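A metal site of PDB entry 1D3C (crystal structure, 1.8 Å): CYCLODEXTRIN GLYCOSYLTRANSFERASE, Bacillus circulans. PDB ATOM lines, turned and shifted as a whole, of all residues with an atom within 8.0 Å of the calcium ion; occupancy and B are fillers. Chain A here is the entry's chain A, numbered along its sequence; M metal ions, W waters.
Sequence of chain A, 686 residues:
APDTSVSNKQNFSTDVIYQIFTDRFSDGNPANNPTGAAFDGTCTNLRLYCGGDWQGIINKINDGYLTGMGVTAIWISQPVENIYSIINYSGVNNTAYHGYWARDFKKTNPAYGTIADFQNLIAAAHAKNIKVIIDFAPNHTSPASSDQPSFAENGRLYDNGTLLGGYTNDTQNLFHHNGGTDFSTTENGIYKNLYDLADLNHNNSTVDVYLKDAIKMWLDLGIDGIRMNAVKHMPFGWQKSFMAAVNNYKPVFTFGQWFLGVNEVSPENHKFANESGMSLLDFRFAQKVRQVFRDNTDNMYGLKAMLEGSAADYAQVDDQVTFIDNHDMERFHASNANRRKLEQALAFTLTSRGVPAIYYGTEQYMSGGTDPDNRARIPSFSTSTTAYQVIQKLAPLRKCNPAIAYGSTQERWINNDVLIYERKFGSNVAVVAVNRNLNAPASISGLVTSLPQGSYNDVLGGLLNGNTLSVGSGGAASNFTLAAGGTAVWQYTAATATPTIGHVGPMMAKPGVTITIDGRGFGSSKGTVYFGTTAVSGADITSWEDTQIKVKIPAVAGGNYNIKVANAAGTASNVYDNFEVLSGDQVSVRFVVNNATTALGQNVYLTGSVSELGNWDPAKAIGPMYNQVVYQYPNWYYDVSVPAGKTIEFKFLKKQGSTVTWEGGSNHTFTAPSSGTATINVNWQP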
ATOM      1  N   THR A  22      12.878 -12.593 -15.658  1.00  0.00           N
ATOM      2  CA  THR A  22      14.336 -12.450 -15.701  1.00  0.00           C
ATOM      3  C   THR A  22      15.127 -13.370 -14.777  1.00  0.00           C
ATOM      4  O   THR A  22      16.097 -13.989 -15.188  1.00  0.00           O
ATOM      5  CB  THR A  22      14.770 -10.985 -15.483  1.00  0.00           C
ATOM      6  OG1 THR A  22      14.071 -10.133 -16.405  1.00  0.00           O
ATOM      7  CG2 THR A  22      16.270 -10.829 -15.691  1.00  0.00           C
ATOM      8  N   ASP A  23      14.690 -13.457 -13.528  1.00  0.00           N
ATOM      9  CA  ASP A  23      15.385 -14.269 -12.536  1.00  0.00           C
ATOM     10  C   ASP A  23      15.274 -15.782 -12.771  1.00  0.00           C
ATOM     11  O   ASP A  23      16.107 -16.558 -12.293  1.00  0.00           O
ATOM     12  CB  ASP A  23      14.900 -13.935 -11.131  1.00  0.00           C
ATOM     13  CG  ASP A  23      15.688 -14.632 -10.054  1.00  0.00           C
ATOM     14  OD1 ASP A  23      16.905 -14.386  -9.952  1.00  0.00           O
ATOM     15  OD2 ASP A  23      15.090 -15.471  -9.339  1.00  0.00           O
ATOM     16  N   SER A  26      17.655 -17.396 -17.302  1.00  0.00           N
ATOM     17  CA  SER A  26      19.029 -17.876 -17.426  1.00  0.00           C
ATOM     18  C   SER A  26      20.026 -16.970 -16.722  1.00  0.00           C
ATOM     19  O   SER A  26      20.082 -15.775 -16.977  1.00  0.00           O
ATOM     20  CB  SER A  26      19.419 -18.044 -18.890  1.00  0.00           C
ATOM     21  OG  SER A  26      20.769 -18.454 -19.019  1.00  0.00           O
ATOM     22  N   ASP A  27      20.812 -17.556 -15.823  1.00  0.00           N
ATOM     23  CA  ASP A  27      21.831 -16.815 -15.091  1.00  0.00           C
ATOM     24  C   ASP A  27      23.072 -16.749 -15.956  1.00  0.00           C
ATOM     25  O   ASP A  27      23.900 -17.673 -15.946  1.00  0.00           O
ATOM     26  CB  ASP A  27      22.167 -17.522 -13.751  1.00  0.00           C
ATOM     27  CG  ASP A  27      23.241 -16.788 -12.963  1.00  0.00           C
ATOM     28  OD1 ASP A  27      23.592 -15.674 -13.361  1.00  0.00           O
ATOM     29  OD2 ASP A  27      23.725 -17.348 -11.954  1.00  0.00           O
ATOM     30  N   GLY A  28      23.184 -15.683 -16.739  1.00  0.00           N
ATOM     31  CA  GLY A  28      24.314 -15.503 -17.634  1.00  0.00           C
ATOM     32  C   GLY A  28      25.543 -14.948 -16.931  1.00  0.00           C
ATOM     33  O   GLY A  28      26.645 -15.007 -17.462  1.00  0.00           O
ATOM     34  N   ASN A  29      25.349 -14.399 -15.735  1.00  0.00           N
ATOM     35  CA  ASN A  29      26.471 -13.825 -14.996  1.00  0.00           C
ATOM     36  C   ASN A  29      26.361 -14.086 -13.495  1.00  0.00           C
ATOM     37  O   ASN A  29      25.702 -13.333 -12.785  1.00  0.00           O
ATOM     38  CB  ASN A  29      26.578 -12.327 -15.287  1.00  0.00           C
ATOM     39  CG  ASN A  29      27.658 -11.644 -14.471  1.00  0.00           C
ATOM     40  OD1 ASN A  29      28.577 -12.290 -13.967  1.00  0.00           O
ATOM     41  ND2 ASN A  29      27.556 -10.325 -14.344  1.00  0.00           N
ATOM     42  N   PRO A  30      26.994 -15.148 -13.039  1.00  0.00           N
ATOM     43  CA  PRO A  30      26.957 -15.528 -11.634  1.00  0.00           C
ATOM     44  C   PRO A  30      27.528 -14.456 -10.699  1.00  0.00           C
ATOM     45  O   PRO A  30      27.213 -14.417  -9.519  1.00  0.00           O
ATOM     46  CB  PRO A  30      27.808 -16.807 -11.569  1.00  0.00           C
ATOM     47  CG  PRO A  30      28.376 -17.026 -12.899  1.00  0.00           C
ATOM     48  CD  PRO A  30      27.864 -16.011 -13.861  1.00  0.00           C
ATOM     49  N   ALA A  31      28.361 -13.578 -11.250  1.00  0.00           N
ATOM     50  CA  ALA A  31      28.998 -12.532 -10.455  1.00  0.00           C
ATOM     51  C   ALA A  31      28.021 -11.498  -9.887  1.00  0.00           C
ATOM     52  O   ALA A  31      28.339 -10.815  -8.914  1.00  0.00           O
ATOM     53  CB  ALA A  31      30.091 -11.851 -11.255  1.00  0.00           C
ATOM     54  N   ASN A  32      26.844 -11.371 -10.487  1.00  0.00           N
ATOM     55  CA  ASN A  32      25.872 -10.402  -9.991  1.00  0.00           C
ATOM     56  C   ASN A  32      24.770 -11.040  -9.153  1.00  0.00           C
ATOM     57  O   ASN A  32      23.816 -10.372  -8.781  1.00  0.00           O
ATOM     58  CB  ASN A  32      25.277  -9.564 -11.131  1.00  0.00           C
ATOM     59  CG  ASN A  32      24.563 -10.419 -12.176  1.00  0.00           C
ATOM     60  OD1 ASN A  32      23.999 -11.431 -11.824  1.00  0.00           O
ATOM     61  ND2 ASN A  32      24.605 -10.061 -13.382  1.00  0.00           N
ATOM     62  N   ASN A  33      24.909 -12.327  -8.855  1.00  0.00           N
ATOM     63  CA  ASN A  33      23.907 -13.030  -8.058  1.00  0.00           C
ATOM     64  C   ASN A  33      23.905 -12.472  -6.644  1.00  0.00           C
ATOM     65  O   ASN A  33      24.948 -12.277  -6.053  1.00  0.00           O
ATOM     66  CB  ASN A  33      24.222 -14.525  -7.995  1.00  0.00           C
ATOM     67  CG  ASN A  33      24.054 -15.219  -9.337  1.00  0.00           C
ATOM     68  OD1 ASN A  33      23.518 -14.632 -10.281  1.00  0.00           O
ATOM     69  ND2 ASN A  33      24.513 -16.464  -9.420  1.00  0.00           N
ATOM     70  N   PRO A  34      22.721 -12.307  -6.066  1.00  0.00           N
ATOM     71  CA  PRO A  34      22.641 -11.888  -4.685  1.00  0.00           C
ATOM     72  C   PRO A  34      23.229 -13.034  -3.879  1.00  0.00           C
ATOM     73  O   PRO A  34      23.500 -14.106  -4.416  1.00  0.00           O
ATOM     74  CB  PRO A  34      21.152 -11.780  -4.445  1.00  0.00           C
ATOM     75  CG  PRO A  34      20.613 -11.326  -5.756  1.00  0.00           C
ATOM     76  CD  PRO A  34      21.521 -11.912  -6.827  1.00  0.00           C
ATOM     77  N   PHE A  39      19.465 -15.642  -1.662  1.00  0.00           N
ATOM     78  CA  PHE A  39      19.781 -16.409  -2.843  1.00  0.00           C
ATOM     79  C   PHE A  39      19.681 -17.927  -2.726  1.00  0.00           C
ATOM     80  O   PHE A  39      20.053 -18.514  -1.716  1.00  0.00           O
ATOM     81  CB  PHE A  39      21.172 -16.026  -3.346  1.00  0.00           C
ATOM     82  CG  PHE A  39      21.578 -16.720  -4.619  1.00  0.00           C
ATOM     83  CD1 PHE A  39      21.094 -16.283  -5.838  1.00  0.00           C
ATOM     84  CD2 PHE A  39      22.433 -17.800  -4.584  1.00  0.00           C
ATOM     85  CE1 PHE A  39      21.470 -16.911  -7.006  1.00  0.00           C
ATOM     86  CE2 PHE A  39      22.795 -18.432  -5.751  1.00  0.00           C
ATOM     87  CZ  PHE A  39      22.324 -17.988  -6.962  1.00  0.00           C
ATOM     88  N   TYR A  49      16.138 -15.121  -4.909  1.00  0.00           N
ATOM     89  CA  TYR A  49      16.768 -14.912  -6.204  1.00  0.00           C
ATOM     90  C   TYR A  49      17.369 -16.212  -6.662  1.00  0.00           C
ATOM     91  O   TYR A  49      17.978 -16.942  -5.880  1.00  0.00           O
ATOM     92  CB  TYR A  49      17.881 -13.871  -6.093  1.00  0.00           C
ATOM     93  CG  TYR A  49      17.419 -12.441  -6.248  1.00  0.00           C
ATOM     94  CD1 TYR A  49      17.391 -11.829  -7.492  1.00  0.00           C
ATOM     95  CD2 TYR A  49      17.031 -11.690  -5.145  1.00  0.00           C
ATOM     96  CE1 TYR A  49      16.999 -10.513  -7.638  1.00  0.00           C
ATOM     97  CE2 TYR A  49      16.621 -10.384  -5.277  1.00  0.00           C
ATOM     98  CZ  TYR A  49      16.603  -9.800  -6.522  1.00  0.00           C
ATOM     99  OH  TYR A  49      16.206  -8.489  -6.655  1.00  0.00           O
ATOM    100  N   CYS A  50      17.220 -16.517  -7.944  1.00  0.00           N
ATOM    101  CA  CYS A  50      17.773 -17.730  -8.486  1.00  0.00           C
ATOM    102  C   CYS A  50      19.012 -17.436  -9.338  1.00  0.00           C
ATOM    103  O   CYS A  50      19.808 -18.335  -9.624  1.00  0.00           O
ATOM    104  CB  CYS A  50      16.721 -18.488  -9.275  1.00  0.00           C
ATOM    105  SG  CYS A  50      15.452 -19.256  -8.218  1.00  0.00           S
ATOM    106  N   GLY A  51      19.194 -16.169  -9.705  1.00  0.00           N
ATOM    107  CA  GLY A  51      20.388 -15.765 -10.448  1.00  0.00           C
ATOM    108  C   GLY A  51      20.170 -15.386 -11.915  1.00  0.00           C
ATOM    109  O   GLY A  51      21.096 -14.968 -12.596  1.00  0.00           O
ATOM    110  N   GLY A  52      18.939 -15.544 -12.400  1.00  0.00           N
ATOM    111  CA  GLY A  52      18.621 -15.215 -13.784  1.00  0.00           C
ATOM    112  C   GLY A  52      18.857 -13.737 -14.047  1.00  0.00           C
ATOM    113  O   GLY A  52      18.421 -12.881 -13.270  1.00  0.00           O
ATOM    114  N   ASP A  53      19.547 -13.422 -15.137  1.00  0.00           N
ATOM    115  CA  ASP A  53      19.861 -12.033 -15.443  1.00  0.00           C
ATOM    116  C   ASP A  53      19.764 -11.684 -16.921  1.00  0.00           C
ATOM    117  O   ASP A  53      19.376 -12.502 -17.748  1.00  0.00           O
ATOM    118  CB  ASP A  53      21.253 -11.698 -14.928  1.00  0.00           C
ATOM    119  CG  ASP A  53      22.285 -12.691 -15.373  1.00  0.00           C
ATOM    120  OD1 ASP A  53      22.174 -13.181 -16.503  1.00  0.00           O
ATOM    121  OD2 ASP A  53      23.180 -13.032 -14.555  1.00  0.00           O
ATOM    122  N   TRP A  54      20.144 -10.446 -17.227  1.00  0.00           N
ATOM    123  CA  TRP A  54      20.104  -9.924 -18.576  1.00  0.00           C
ATOM    124  C   TRP A  54      21.124 -10.580 -19.496  1.00  0.00           C
ATOM    125  O   TRP A  54      20.848 -10.784 -20.675  1.00  0.00           O
ATOM    126  CB  TRP A  54      20.273  -8.406 -18.567  1.00  0.00           C
ATOM    127  CG  TRP A  54      19.107  -7.690 -17.966  1.00  0.00           C
ATOM    128  CD1 TRP A  54      17.817  -8.142 -17.897  1.00  0.00           C
ATOM    129  CD2 TRP A  54      19.123  -6.405 -17.327  1.00  0.00           C
ATOM    130  NE1 TRP A  54      17.027  -7.215 -17.270  1.00  0.00           N
ATOM    131  CE2 TRP A  54      17.799  -6.138 -16.913  1.00  0.00           C
ATOM    132  CE3 TRP A  54      20.106  -5.459 -17.074  1.00  0.00           C
ATOM    133  CZ2 TRP A  54      17.442  -4.968 -16.261  1.00  0.00           C
ATOM    134  CZ3 TRP A  54      19.749  -4.290 -16.422  1.00  0.00           C
ATOM    135  CH2 TRP A  54      18.426  -4.050 -16.019  1.00  0.00           C
ATOM    136  N   GLN A  55      22.291 -10.927 -18.964  1.00  0.00           N
ATOM    137  CA  GLN A  55      23.318 -11.582 -19.778  1.00  0.00           C
ATOM    138  C   GLN A  55      22.828 -12.952 -20.232  1.00  0.00           C
ATOM    139  O   GLN A  55      23.165 -13.415 -21.322  1.00  0.00           O
ATOM    140  CB  GLN A  55      24.632 -11.713 -19.007  1.00  0.00           C
ATOM    141  CG  GLN A  55      25.698 -12.506 -19.759  1.00  0.00           C
ATOM    142  CD  GLN A  55      26.178 -11.799 -21.022  1.00  0.00           C
ATOM    143  OE1 GLN A  55      26.875 -10.789 -20.948  1.00  0.00           O
ATOM    144  NE2 GLN A  55      25.827 -12.343 -22.172  1.00  0.00           N
ATOM    145  N   GLY A  56      22.045 -13.589 -19.376  1.00  0.00           N
ATOM    146  CA  GLY A  56      21.485 -14.897 -19.693  1.00  0.00           C
ATOM    147  C   GLY A  56      20.499 -14.748 -20.835  1.00  0.00           C
ATOM    148  O   GLY A  56      20.424 -15.603 -21.725  1.00  0.00           O
ATOM    149  N   PRO A 110      20.663  -4.384  -9.839  1.00  0.00           N
ATOM    150  CA  PRO A 110      21.987  -5.000  -9.956  1.00  0.00           C
ATOM    151  C   PRO A 110      21.934  -6.493 -10.221  1.00  0.00           C
ATOM    152  O   PRO A 110      22.767  -7.049 -10.930  1.00  0.00           O
ATOM    153  CB  PRO A 110      22.608  -4.723  -8.594  1.00  0.00           C
ATOM    154  CG  PRO A 110      21.929  -3.495  -8.120  1.00  0.00           C
ATOM    155  CD  PRO A 110      20.515  -3.634  -8.578  1.00  0.00           C
ATOM    156  N   ALA A 111      20.963  -7.164  -9.616  1.00  0.00           N
ATOM    157  CA  ALA A 111      20.820  -8.604  -9.793  1.00  0.00           C
ATOM    158  C   ALA A 111      20.650  -8.924 -11.272  1.00  0.00           C
ATOM    159  O   ALA A 111      21.237  -9.873 -11.782  1.00  0.00           O
ATOM    160  CB  ALA A 111      19.630  -9.135  -9.004  1.00  0.00           C
ATOM    161  N   TYR A 112      19.866  -8.110 -11.966  1.00  0.00           N
ATOM    162  CA  TYR A 112      19.618  -8.289 -13.389  1.00  0.00           C
ATOM    163  C   TYR A 112      20.846  -7.879 -14.198  1.00  0.00           C
ATOM    164  O   TYR A 112      21.282  -8.582 -15.106  1.00  0.00           O
ATOM    165  CB  TYR A 112      18.409  -7.478 -13.833  1.00  0.00           C
ATOM    166  CG  TYR A 112      17.074  -7.855 -13.173  1.00  0.00           C
ATOM    167  CD1 TYR A 112      16.868  -9.122 -12.646  1.00  0.00           C
ATOM    168  CD2 TYR A 112      16.024  -6.945 -13.134  1.00  0.00           C
ATOM    169  CE1 TYR A 112      15.642  -9.457 -12.077  1.00  0.00           C
ATOM    170  CE2 TYR A 112      14.815  -7.263 -12.561  1.00  0.00           C
ATOM    171  CZ  TYR A 112      14.623  -8.526 -12.035  1.00  0.00           C
ATOM    172  OH  TYR A 112      13.410  -8.835 -11.476  1.00  0.00           O
ATOM    173  N   GLY A 113      21.405  -6.719 -13.870  1.00  0.00           N
ATOM    174  CA  GLY A 113      22.580  -6.219 -14.572  1.00  0.00           C
ATOM    175  C   GLY A 113      22.762  -4.728 -14.362  1.00  0.00           C
ATOM    176  O   GLY A 113      22.031  -4.099 -13.605  1.00  0.00           O
HETATM  177 CA    CA M   1      23.179 -13.738 -12.296  1.00  0.00          CA
HETATM  178  O   HOH W   1      21.605 -12.376 -10.842  1.00  0.00           O
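ND2 of Asn 33 lies close to O of Pro 30 (3.4 Å).
The backbone NH (N) of Gly 28 is in hydrogen-bond range of the side-chain carboxylate (OD1) of Asp 53, at 2.7 Å.
The backbone carbonyl oxygen (O) of Ser 26 lies within hydrogen-bond range of the backbone NH (N) of Asp 53.
The side-chain carboxylate (OD1) of Asp 53 sits close to the backbone NH (N) of Gln 55 (3.3 Å).
The backbone NH of Asp 53 sits at hydrogen-bond distance from the backbone carbonyl oxygen of Thr 22 (3.5 Å).
N of Gly 51 lies within hydrogen-bond range of OD1 of Asp 23 (2.9 Å).
The side-chain amide oxygen (OD1) of Asn 32 lies close to the backbone carbonyl oxygen (O) of Ala 111 (3.2 Å).
The backbone NH (N) of Ala 31 sits at hydrogen-bond distance from the side-chain amide oxygen (OD1) of Asn 29 (3.0 Å).
Of the 24 residues printed, 6 come within 4 Å of the calcium ion.
The calcium ion is bound by OD1 of Asn 33 (2.2 Å), OD1 of Asp 27 (2.2 Å), OD2 of Asp 53 (2.4 Å), O of Gly 51 (2.4 Å), OD1 of Asn 32 (2.5 Å), water W1 (2.5 Å) and O of Asn 29 (2.6 Å).
The calcium ion has seven donor atoms within binding distance.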
